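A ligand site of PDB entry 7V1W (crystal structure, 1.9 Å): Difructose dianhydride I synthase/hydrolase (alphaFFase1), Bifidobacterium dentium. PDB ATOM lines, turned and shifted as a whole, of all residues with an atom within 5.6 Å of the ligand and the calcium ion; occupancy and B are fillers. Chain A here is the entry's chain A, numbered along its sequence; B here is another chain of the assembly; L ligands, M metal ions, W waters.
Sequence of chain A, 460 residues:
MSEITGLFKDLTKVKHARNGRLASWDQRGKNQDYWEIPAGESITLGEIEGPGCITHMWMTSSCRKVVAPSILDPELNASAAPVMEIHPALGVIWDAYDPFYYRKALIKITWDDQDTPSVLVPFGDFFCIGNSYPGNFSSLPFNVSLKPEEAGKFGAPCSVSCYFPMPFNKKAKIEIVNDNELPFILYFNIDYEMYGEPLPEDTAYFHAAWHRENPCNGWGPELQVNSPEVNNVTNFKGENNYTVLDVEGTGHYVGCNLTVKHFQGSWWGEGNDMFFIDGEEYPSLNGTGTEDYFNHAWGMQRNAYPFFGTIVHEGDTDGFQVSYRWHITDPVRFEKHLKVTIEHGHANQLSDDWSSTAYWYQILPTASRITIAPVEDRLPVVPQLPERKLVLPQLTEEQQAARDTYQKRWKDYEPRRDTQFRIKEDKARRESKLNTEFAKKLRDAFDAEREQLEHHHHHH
Gly 289 touches the ligand. Ala 297 touches the ligand (CA to O4, 3.4 Å). Gly 299 touches the ligand. CG2 of Thr 60 of chain B touches O4 of the ligand, at 3.8 Å. CE2 of Tyr 187 of chain B touches O3 of the ligand (3.4 Å). 12 residues have an atom within 4 Å of the ligand: Trp 267, Gly 269, Glu 270, Thr 288, Gly 289, Glu 291, Asp 292, Ala 297, Trp 298, Gly 299, Thr 60 of chain B and Tyr 187 of chain B. The nearest printed residue that does not touch the ligand is Trp 58 of chain B (4.5 Å).
An oxygen (O1) of the ligand is in hydrogen-bond range of the backbone carbonyl oxygen (O) of Gly 269 (3.1 Å). O3 of the ligand sits close to O of Thr 288, at 3.3 Å. N of Trp 298 is in hydrogen-bond range of O4 of the ligand. The indole nitrogen (NE1) of Trp 267 is in hydrogen-bond range of an oxygen (O1) of the ligand (2.9 Å). The side-chain carboxylate (OE2) of Glu 291 sits at hydrogen-bond distance from an oxygen (O5) of the ligand, 2.5 Å away. The side-chain carboxylate (OE2) of Glu 270 lies close to an oxygen (O1) of the ligand, at 3.4 Å. OD2 of Asp 292 is in hydrogen-bond range of O3 of the ligand (2.7 Å).
Water W3 lies within hydrogen-bond range of the side-chain carboxylate (OE1) of Glu 343, a ring nitrogen (ND1) of His 346 and the side-chain amide nitrogen (ND2) of Asn 272. Water W2 bridges the side-chain carboxylate of Glu 270 (2.7 Å) and an oxygen (O3) of the ligand (2.9 Å).
The backbone carbonyl oxygen (O) of Gly 269 lies within hydrogen-bond range of the backbone NH (N) of Thr 290 (2.7 Å). NE1 of Trp 298 sits at hydrogen-bond distance from OG1 of Thr 60 of chain B (2.9 Å). The backbone NH of Gly 289 sits close to the side-chain amide oxygen of Asn 272 (3.4 Å). OD2 of Asp 292 lies within hydrogen-bond range of N of Gly 289 (3.4 Å). The side-chain carboxylate (OE2) of Glu 291 is in hydrogen-bond range of the backbone NH (N) of Gly 299, 2.9 Å away. OE2 of Glu 291 lies within hydrogen-bond range of N of Trp 298, at 3.2 Å. OD2 of Asp 292 sits at hydrogen-bond distance from OG1 of Thr 288 (2.6 Å). O of Thr 60 of chain B is in hydrogen-bond range of N of Tyr 187 of chain B, 2.8 Å away.
The side-chain carboxylate (OD2) of Asp 33 of chain B is bound to the calcium ion (2.3 Å). The calcium ion is bound by the side-chain amide oxygen (OD1) of Asn 272, 2.4 Å away. O of Glu 270 binds the calcium ion (2.4 Å). OD1 of Asn 31 of chain B binds the calcium ion, 2.4 Å away. Water W3 is bound to the calcium ion (2.5 Å). The calcium ion is bound by water W2, 2.6 Å away. The calcium ion is bound by O of Thr 288, at 2.7 Å.
The nearest printed residue that does not touch the calcium ion is Gly 289 (4.2 Å).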
ATOM      1  N   TRP A 267     -10.694 -30.086   9.380  1.00  0.00           N
ATOM      2  CA  TRP A 267     -11.699 -30.074   8.288  1.00  0.00           C
ATOM      3  C   TRP A 267     -11.419 -28.892   7.359  1.00  0.00           C
ATOM      4  O   TRP A 267     -11.282 -27.752   7.845  1.00  0.00           O
ATOM      5  CB  TRP A 267     -13.095 -30.011   8.908  1.00  0.00           C
ATOM      6  CG  TRP A 267     -14.209 -29.802   7.955  1.00  0.00           C
ATOM      7  CD1 TRP A 267     -15.190 -28.862   8.066  1.00  0.00           C
ATOM      8  CD2 TRP A 267     -14.539 -30.574   6.784  1.00  0.00           C
ATOM      9  NE1 TRP A 267     -16.111 -28.999   7.070  1.00  0.00           N
ATOM     10  CE2 TRP A 267     -15.717 -30.023   6.249  1.00  0.00           C
ATOM     11  CE3 TRP A 267     -13.954 -31.659   6.133  1.00  0.00           C
ATOM     12  CZ2 TRP A 267     -16.303 -30.482   5.072  1.00  0.00           C
ATOM     13  CZ3 TRP A 267     -14.561 -32.150   4.994  1.00  0.00           C
ATOM     14  CH2 TRP A 267     -15.717 -31.572   4.472  1.00  0.00           C
ATOM     15  N   GLY A 269     -13.515 -27.751   4.935  1.00  0.00           N
ATOM     16  CA  GLY A 269     -14.723 -27.585   4.114  1.00  0.00           C
ATOM     17  C   GLY A 269     -15.771 -26.658   4.681  1.00  0.00           C
ATOM     18  O   GLY A 269     -16.922 -26.765   4.258  1.00  0.00           O
ATOM     19  N   GLU A 270     -15.406 -25.754   5.579  1.00  0.00           N
ATOM     20  CA  GLU A 270     -16.390 -24.848   6.231  1.00  0.00           C
ATOM     21  C   GLU A 270     -16.743 -23.710   5.270  1.00  0.00           C
ATOM     22  O   GLU A 270     -17.729 -22.995   5.522  1.00  0.00           O
ATOM     23  CB  GLU A 270     -15.843 -24.235   7.517  1.00  0.00           C
ATOM     24  CG  GLU A 270     -15.734 -25.218   8.661  1.00  0.00           C
ATOM     25  CD  GLU A 270     -17.061 -25.701   9.222  1.00  0.00           C
ATOM     26  OE1 GLU A 270     -18.090 -24.967   9.146  1.00  0.00           O
ATOM     27  OE2 GLU A 270     -17.085 -26.847   9.692  1.00  0.00           O
ATOM     28  N   GLY A 271     -15.959 -23.508   4.223  1.00  0.00           N
ATOM     29  CA  GLY A 271     -16.130 -22.356   3.329  1.00  0.00           C
ATOM     30  C   GLY A 271     -17.372 -22.478   2.461  1.00  0.00           C
ATOM     31  O   GLY A 271     -17.700 -23.605   1.986  1.00  0.00           O
ATOM     32  N   ASN A 272     -18.079 -21.364   2.285  1.00  0.00           N
ATOM     33  CA  ASN A 272     -19.353 -21.278   1.536  1.00  0.00           C
ATOM     34  C   ASN A 272     -19.039 -21.066   0.051  1.00  0.00           C
ATOM     35  O   ASN A 272     -18.144 -20.210  -0.277  1.00  0.00           O
ATOM     36  CB  ASN A 272     -20.212 -20.091   1.994  1.00  0.00           C
ATOM     37  CG  ASN A 272     -20.589 -20.108   3.461  1.00  0.00           C
ATOM     38  OD1 ASN A 272     -20.310 -21.073   4.163  1.00  0.00           O
ATOM     39  ND2 ASN A 272     -21.247 -19.044   3.916  1.00  0.00           N
ATOM     40  N   THR A 288     -23.457 -22.439   2.373  1.00  0.00           N
ATOM     41  CA  THR A 288     -23.359 -22.657   3.835  1.00  0.00           C
ATOM     42  C   THR A 288     -22.084 -23.367   4.208  1.00  0.00           C
ATOM     43  O   THR A 288     -21.720 -23.287   5.369  1.00  0.00           O
ATOM     44  CB  THR A 288     -24.607 -23.394   4.322  1.00  0.00           C
ATOM     45  OG1 THR A 288     -24.711 -24.654   3.654  1.00  0.00           O
ATOM     46  CG2 THR A 288     -25.842 -22.571   4.097  1.00  0.00           C
ATOM     47  N   GLY A 289     -21.479 -24.095   3.262  1.00  0.00           N
ATOM     48  CA  GLY A 289     -20.259 -24.878   3.514  1.00  0.00           C
ATOM     49  C   GLY A 289     -19.853 -25.647   2.266  1.00  0.00           C
ATOM     50  O   GLY A 289     -20.624 -25.677   1.287  1.00  0.00           O
ATOM     51  N   THR A 290     -18.650 -26.189   2.235  1.00  0.00           N
ATOM     52  CA  THR A 290     -18.146 -26.804   0.974  1.00  0.00           C
ATOM     53  C   THR A 290     -18.802 -28.183   0.716  1.00  0.00           C
ATOM     54  O   THR A 290     -19.206 -28.429  -0.434  1.00  0.00           O
ATOM     55  CB  THR A 290     -16.624 -26.816   0.924  1.00  0.00           C
ATOM     56  OG1 THR A 290     -16.223 -25.480   1.265  1.00  0.00           O
ATOM     57  CG2 THR A 290     -16.109 -27.199  -0.448  1.00  0.00           C
ATOM     58  N   GLU A 291     -18.903 -29.065   1.730  1.00  0.00           N
ATOM     59  CA  GLU A 291     -19.598 -30.375   1.559  1.00  0.00           C
ATOM     60  C   GLU A 291     -21.068 -30.035   1.300  1.00  0.00           C
ATOM     61  O   GLU A 291     -21.711 -30.757   0.505  1.00  0.00           O
ATOM     62  CB  GLU A 291     -19.354 -31.369   2.709  1.00  0.00           C
ATOM     63  CG  GLU A 291     -20.304 -31.208   3.900  1.00  0.00           C
ATOM     64  CD  GLU A 291     -19.808 -30.177   4.878  1.00  0.00           C
ATOM     65  OE1 GLU A 291     -19.552 -29.025   4.427  1.00  0.00           O
ATOM     66  OE2 GLU A 291     -19.688 -30.517   6.090  1.00  0.00           O
ATOM     67  N   ASP A 292     -21.559 -28.906   1.820  1.00  0.00           N
ATOM     68  CA  ASP A 292     -22.995 -28.573   1.618  1.00  0.00           C
ATOM     69  C   ASP A 292     -23.215 -28.316   0.130  1.00  0.00           C
ATOM     70  O   ASP A 292     -24.238 -28.774  -0.422  1.00  0.00           O
ATOM     71  CB  ASP A 292     -23.454 -27.375   2.456  1.00  0.00           C
ATOM     72  CG  ASP A 292     -23.165 -27.552   3.945  1.00  0.00           C
ATOM     73  OD1 ASP A 292     -22.770 -28.679   4.366  1.00  0.00           O
ATOM     74  OD2 ASP A 292     -23.306 -26.537   4.659  1.00  0.00           O
ATOM     75  N   HIS A 296     -23.431 -33.125   0.444  1.00  0.00           N
ATOM     76  CA  HIS A 296     -23.182 -33.969   1.633  1.00  0.00           C
ATOM     77  C   HIS A 296     -23.448 -33.099   2.883  1.00  0.00           C
ATOM     78  O   HIS A 296     -24.022 -31.983   2.721  1.00  0.00           O
ATOM     79  CB  HIS A 296     -21.800 -34.607   1.538  1.00  0.00           C
ATOM     80  CG  HIS A 296     -21.762 -35.677   0.512  1.00  0.00           C
ATOM     81  ND1 HIS A 296     -20.753 -36.636   0.493  1.00  0.00           N
ATOM     82  CD2 HIS A 296     -22.617 -35.976  -0.495  1.00  0.00           C
ATOM     83  CE1 HIS A 296     -20.990 -37.448  -0.514  1.00  0.00           C
ATOM     84  NE2 HIS A 296     -22.130 -37.082  -1.109  1.00  0.00           N
ATOM     85  N   ALA A 297     -23.111 -33.603   4.066  1.00  0.00           N
ATOM     86  CA  ALA A 297     -23.231 -32.851   5.352  1.00  0.00           C
ATOM     87  C   ALA A 297     -22.337 -33.470   6.412  1.00  0.00           C
ATOM     88  O   ALA A 297     -22.185 -34.728   6.412  1.00  0.00           O
ATOM     89  CB  ALA A 297     -24.677 -32.806   5.787  1.00  0.00           C
ATOM     90  N   TRP A 298     -21.760 -32.625   7.296  1.00  0.00           N
ATOM     91  CA  TRP A 298     -20.915 -33.052   8.442  1.00  0.00           C
ATOM     92  C   TRP A 298     -19.719 -33.815   7.880  1.00  0.00           C
ATOM     93  O   TRP A 298     -19.431 -34.921   8.337  1.00  0.00           O
ATOM     94  CB  TRP A 298     -21.727 -33.906   9.445  1.00  0.00           C
ATOM     95  CG  TRP A 298     -23.108 -33.381   9.677  1.00  0.00           C
ATOM     96  CD1 TRP A 298     -24.249 -33.812   9.078  1.00  0.00           C
ATOM     97  CD2 TRP A 298     -23.477 -32.239  10.468  1.00  0.00           C
ATOM     98  NE1 TRP A 298     -25.316 -33.047   9.472  1.00  0.00           N
ATOM     99  CE2 TRP A 298     -24.874 -32.077  10.322  1.00  0.00           C
ATOM    100  CE3 TRP A 298     -22.786 -31.352  11.297  1.00  0.00           C
ATOM    101  CZ2 TRP A 298     -25.588 -31.063  10.953  1.00  0.00           C
ATOM    102  CZ3 TRP A 298     -23.490 -30.355  11.929  1.00  0.00           C
ATOM    103  CH2 TRP A 298     -24.872 -30.222  11.765  1.00  0.00           C
ATOM    104  N   GLY A 299     -19.094 -33.270   6.848  1.00  0.00           N
ATOM    105  CA  GLY A 299     -18.061 -34.001   6.115  1.00  0.00           C
ATOM    106  C   GLY A 299     -18.568 -34.455   4.760  1.00  0.00           C
ATOM    107  O   GLY A 299     -19.771 -34.318   4.474  1.00  0.00           O
ATOM    108  N   GLU A 343     -15.301 -20.115  -0.411  1.00  0.00           N
ATOM    109  CA  GLU A 343     -14.372 -19.681   0.642  1.00  0.00           C
ATOM    110  C   GLU A 343     -13.436 -20.864   0.923  1.00  0.00           C
ATOM    111  O   GLU A 343     -13.953 -22.002   1.066  1.00  0.00           O
ATOM    112  CB  GLU A 343     -15.071 -19.304   1.932  1.00  0.00           C
ATOM    113  CG  GLU A 343     -16.174 -18.277   1.824  1.00  0.00           C
ATOM    114  CD  GLU A 343     -16.722 -18.064   3.229  1.00  0.00           C
ATOM    115  OE1 GLU A 343     -17.446 -18.960   3.715  1.00  0.00           O
ATOM    116  OE2 GLU A 343     -16.352 -17.057   3.870  1.00  0.00           O
ATOM    117  N   HIS A 346     -13.598 -21.319   6.207  1.00  0.00           N
ATOM    118  CA  HIS A 346     -14.448 -20.188   6.638  1.00  0.00           C
ATOM    119  C   HIS A 346     -13.646 -18.886   6.462  1.00  0.00           C
ATOM    120  O   HIS A 346     -12.508 -18.785   7.005  1.00  0.00           O
ATOM    121  CB  HIS A 346     -14.913 -20.344   8.092  1.00  0.00           C
ATOM    122  CG  HIS A 346     -15.591 -19.086   8.495  1.00  0.00           C
ATOM    123  ND1 HIS A 346     -16.689 -18.621   7.809  1.00  0.00           N
ATOM    124  CD2 HIS A 346     -15.205 -18.104   9.333  1.00  0.00           C
ATOM    125  CE1 HIS A 346     -17.019 -17.420   8.284  1.00  0.00           C
ATOM    126  NE2 HIS A 346     -16.106 -17.069   9.224  1.00  0.00           N
ATOM    127  N   LYS B  30     -20.438 -14.659   9.153  1.00  0.00           N
ATOM    128  CA  LYS B  30     -19.605 -15.489  10.060  1.00  0.00           C
ATOM    129  C   LYS B  30     -19.849 -16.966   9.700  1.00  0.00           C
ATOM    130  O   LYS B  30     -20.283 -17.215   8.579  1.00  0.00           O
ATOM    131  CB  LYS B  30     -19.870 -15.127  11.527  1.00  0.00           C
ATOM    132  CG  LYS B  30     -19.570 -13.676  11.870  1.00  0.00           C
ATOM    133  CD  LYS B  30     -19.856 -13.251  13.283  1.00  0.00           C
ATOM    134  CE  LYS B  30     -19.455 -11.807  13.539  1.00  0.00           C
ATOM    135  NZ  LYS B  30     -19.314 -11.560  14.988  1.00  0.00           N
ATOM    136  N   ASN B  31     -19.565 -17.906  10.584  1.00  0.00           N
ATOM    137  CA  ASN B  31     -19.627 -19.341  10.204  1.00  0.00           C
ATOM    138  C   ASN B  31     -20.782 -20.067  10.906  1.00  0.00           C
ATOM    139  O   ASN B  31     -20.660 -21.320  11.102  1.00  0.00           O
ATOM    140  CB  ASN B  31     -18.289 -20.030  10.424  1.00  0.00           C
ATOM    141  CG  ASN B  31     -18.198 -21.324   9.630  1.00  0.00           C
ATOM    142  OD1 ASN B  31     -18.752 -21.458   8.522  1.00  0.00           O
ATOM    143  ND2 ASN B  31     -17.555 -22.298  10.228  1.00  0.00           N
ATOM    144  N   ASP B  33     -23.831 -20.870   9.455  1.00  0.00           N
ATOM    145  CA  ASP B  33     -24.600 -20.897   8.181  1.00  0.00           C
ATOM    146  C   ASP B  33     -25.805 -21.837   8.334  1.00  0.00           C
ATOM    147  O   ASP B  33     -26.186 -22.476   7.350  1.00  0.00           O
ATOM    148  CB  ASP B  33     -23.688 -21.232   7.016  1.00  0.00           C
ATOM    149  CG  ASP B  33     -22.543 -20.242   6.908  1.00  0.00           C
ATOM    150  OD1 ASP B  33     -22.775 -19.045   6.515  1.00  0.00           O
ATOM    151  OD2 ASP B  33     -21.442 -20.637   7.256  1.00  0.00           O
ATOM    152  N   TRP B  58     -31.355 -28.702  -0.878  1.00  0.00           N
ATOM    153  CA  TRP B  58     -30.438 -29.446   0.019  1.00  0.00           C
ATOM    154  C   TRP B  58     -30.731 -28.988   1.445  1.00  0.00           C
ATOM    155  O   TRP B  58     -30.972 -27.784   1.665  1.00  0.00           O
ATOM    156  CB  TRP B  58     -28.977 -29.214  -0.365  1.00  0.00           C
ATOM    157  CG  TRP B  58     -28.012 -29.722   0.667  1.00  0.00           C
ATOM    158  CD1 TRP B  58     -27.482 -30.981   0.746  1.00  0.00           C
ATOM    159  CD2 TRP B  58     -27.530 -29.001   1.804  1.00  0.00           C
ATOM    160  NE1 TRP B  58     -26.664 -31.075   1.841  1.00  0.00           N
ATOM    161  CE2 TRP B  58     -26.668 -29.872   2.507  1.00  0.00           C
ATOM    162  CE3 TRP B  58     -27.672 -27.672   2.256  1.00  0.00           C
ATOM    163  CZ2 TRP B  58     -25.996 -29.479   3.679  1.00  0.00           C
ATOM    164  CZ3 TRP B  58     -27.027 -27.298   3.414  1.00  0.00           C
ATOM    165  CH2 TRP B  58     -26.208 -28.184   4.123  1.00  0.00           C
ATOM    166  N   THR B  60     -29.506 -30.127   5.811  1.00  0.00           N
ATOM    167  CA  THR B  60     -29.161 -31.050   6.911  1.00  0.00           C
ATOM    168  C   THR B  60     -29.668 -30.457   8.207  1.00  0.00           C
ATOM    169  O   THR B  60     -30.129 -29.285   8.228  1.00  0.00           O
ATOM    170  CB  THR B  60     -27.679 -31.417   6.884  1.00  0.00           C
ATOM    171  OG1 THR B  60     -27.580 -32.576   7.697  1.00  0.00           O
ATOM    172  CG2 THR B  60     -26.787 -30.293   7.339  1.00  0.00           C
ATOM    173  N   TYR B 187     -29.629 -26.498   8.372  1.00  0.00           N
ATOM    174  CA  TYR B 187     -28.892 -25.947   7.205  1.00  0.00           C
ATOM    175  C   TYR B 187     -29.786 -26.117   5.989  1.00  0.00           C
ATOM    176  O   TYR B 187     -30.361 -27.233   5.825  1.00  0.00           O
ATOM    177  CB  TYR B 187     -27.609 -26.725   6.957  1.00  0.00           C
ATOM    178  CG  TYR B 187     -26.490 -26.445   7.917  1.00  0.00           C
ATOM    179  CD1 TYR B 187     -26.425 -27.040   9.165  1.00  0.00           C
ATOM    180  CD2 TYR B 187     -25.467 -25.585   7.543  1.00  0.00           C
ATOM    181  CE1 TYR B 187     -25.358 -26.792  10.021  1.00  0.00           C
ATOM    182  CE2 TYR B 187     -24.407 -25.332   8.376  1.00  0.00           C
ATOM    183  CZ  TYR B 187     -24.353 -25.936   9.621  1.00  0.00           C
ATOM    184  OH  TYR B 187     -23.287 -25.624  10.412  1.00  0.00           O
HETATM  185  O1  LIG L   1     -18.558 -27.540   6.715  1.00  0.00           O
HETATM  186  C1  LIG L   1     -19.641 -27.568   7.709  1.00  0.00           C
HETATM  187  C2  LIG L   1     -19.649 -28.724   8.725  1.00  0.00           C
HETATM  188  O2  LIG L   1     -21.015 -29.198   8.851  1.00  0.00           O
HETATM  189  C3  LIG L   1     -21.063 -27.612   7.158  1.00  0.00           C
HETATM  190  O3  LIG L   1     -21.563 -26.301   6.747  1.00  0.00           O
HETATM  191  C4  LIG L   1     -21.904 -28.231   8.303  1.00  0.00           C
HETATM  192  C5  LIG L   1     -23.224 -28.868   7.916  1.00  0.00           C
HETATM  193  O4  LIG L   1     -23.000 -29.918   6.966  1.00  0.00           O
HETATM  194  O5  LIG L   1     -18.788 -29.828   8.362  1.00  0.00           O
HETATM  195 CA    CA M   1     -19.685 -21.861   6.335  1.00  0.00          CA
HETATM  196  O   HOH W   1     -20.964 -28.276  11.483  1.00  0.00           O
HETATM  197  O   HOH W   2     -20.154 -23.993   7.659  1.00  0.00           O
HETATM  198  O   HOH W   3     -18.566 -19.590   6.052  1.00  0.00           O
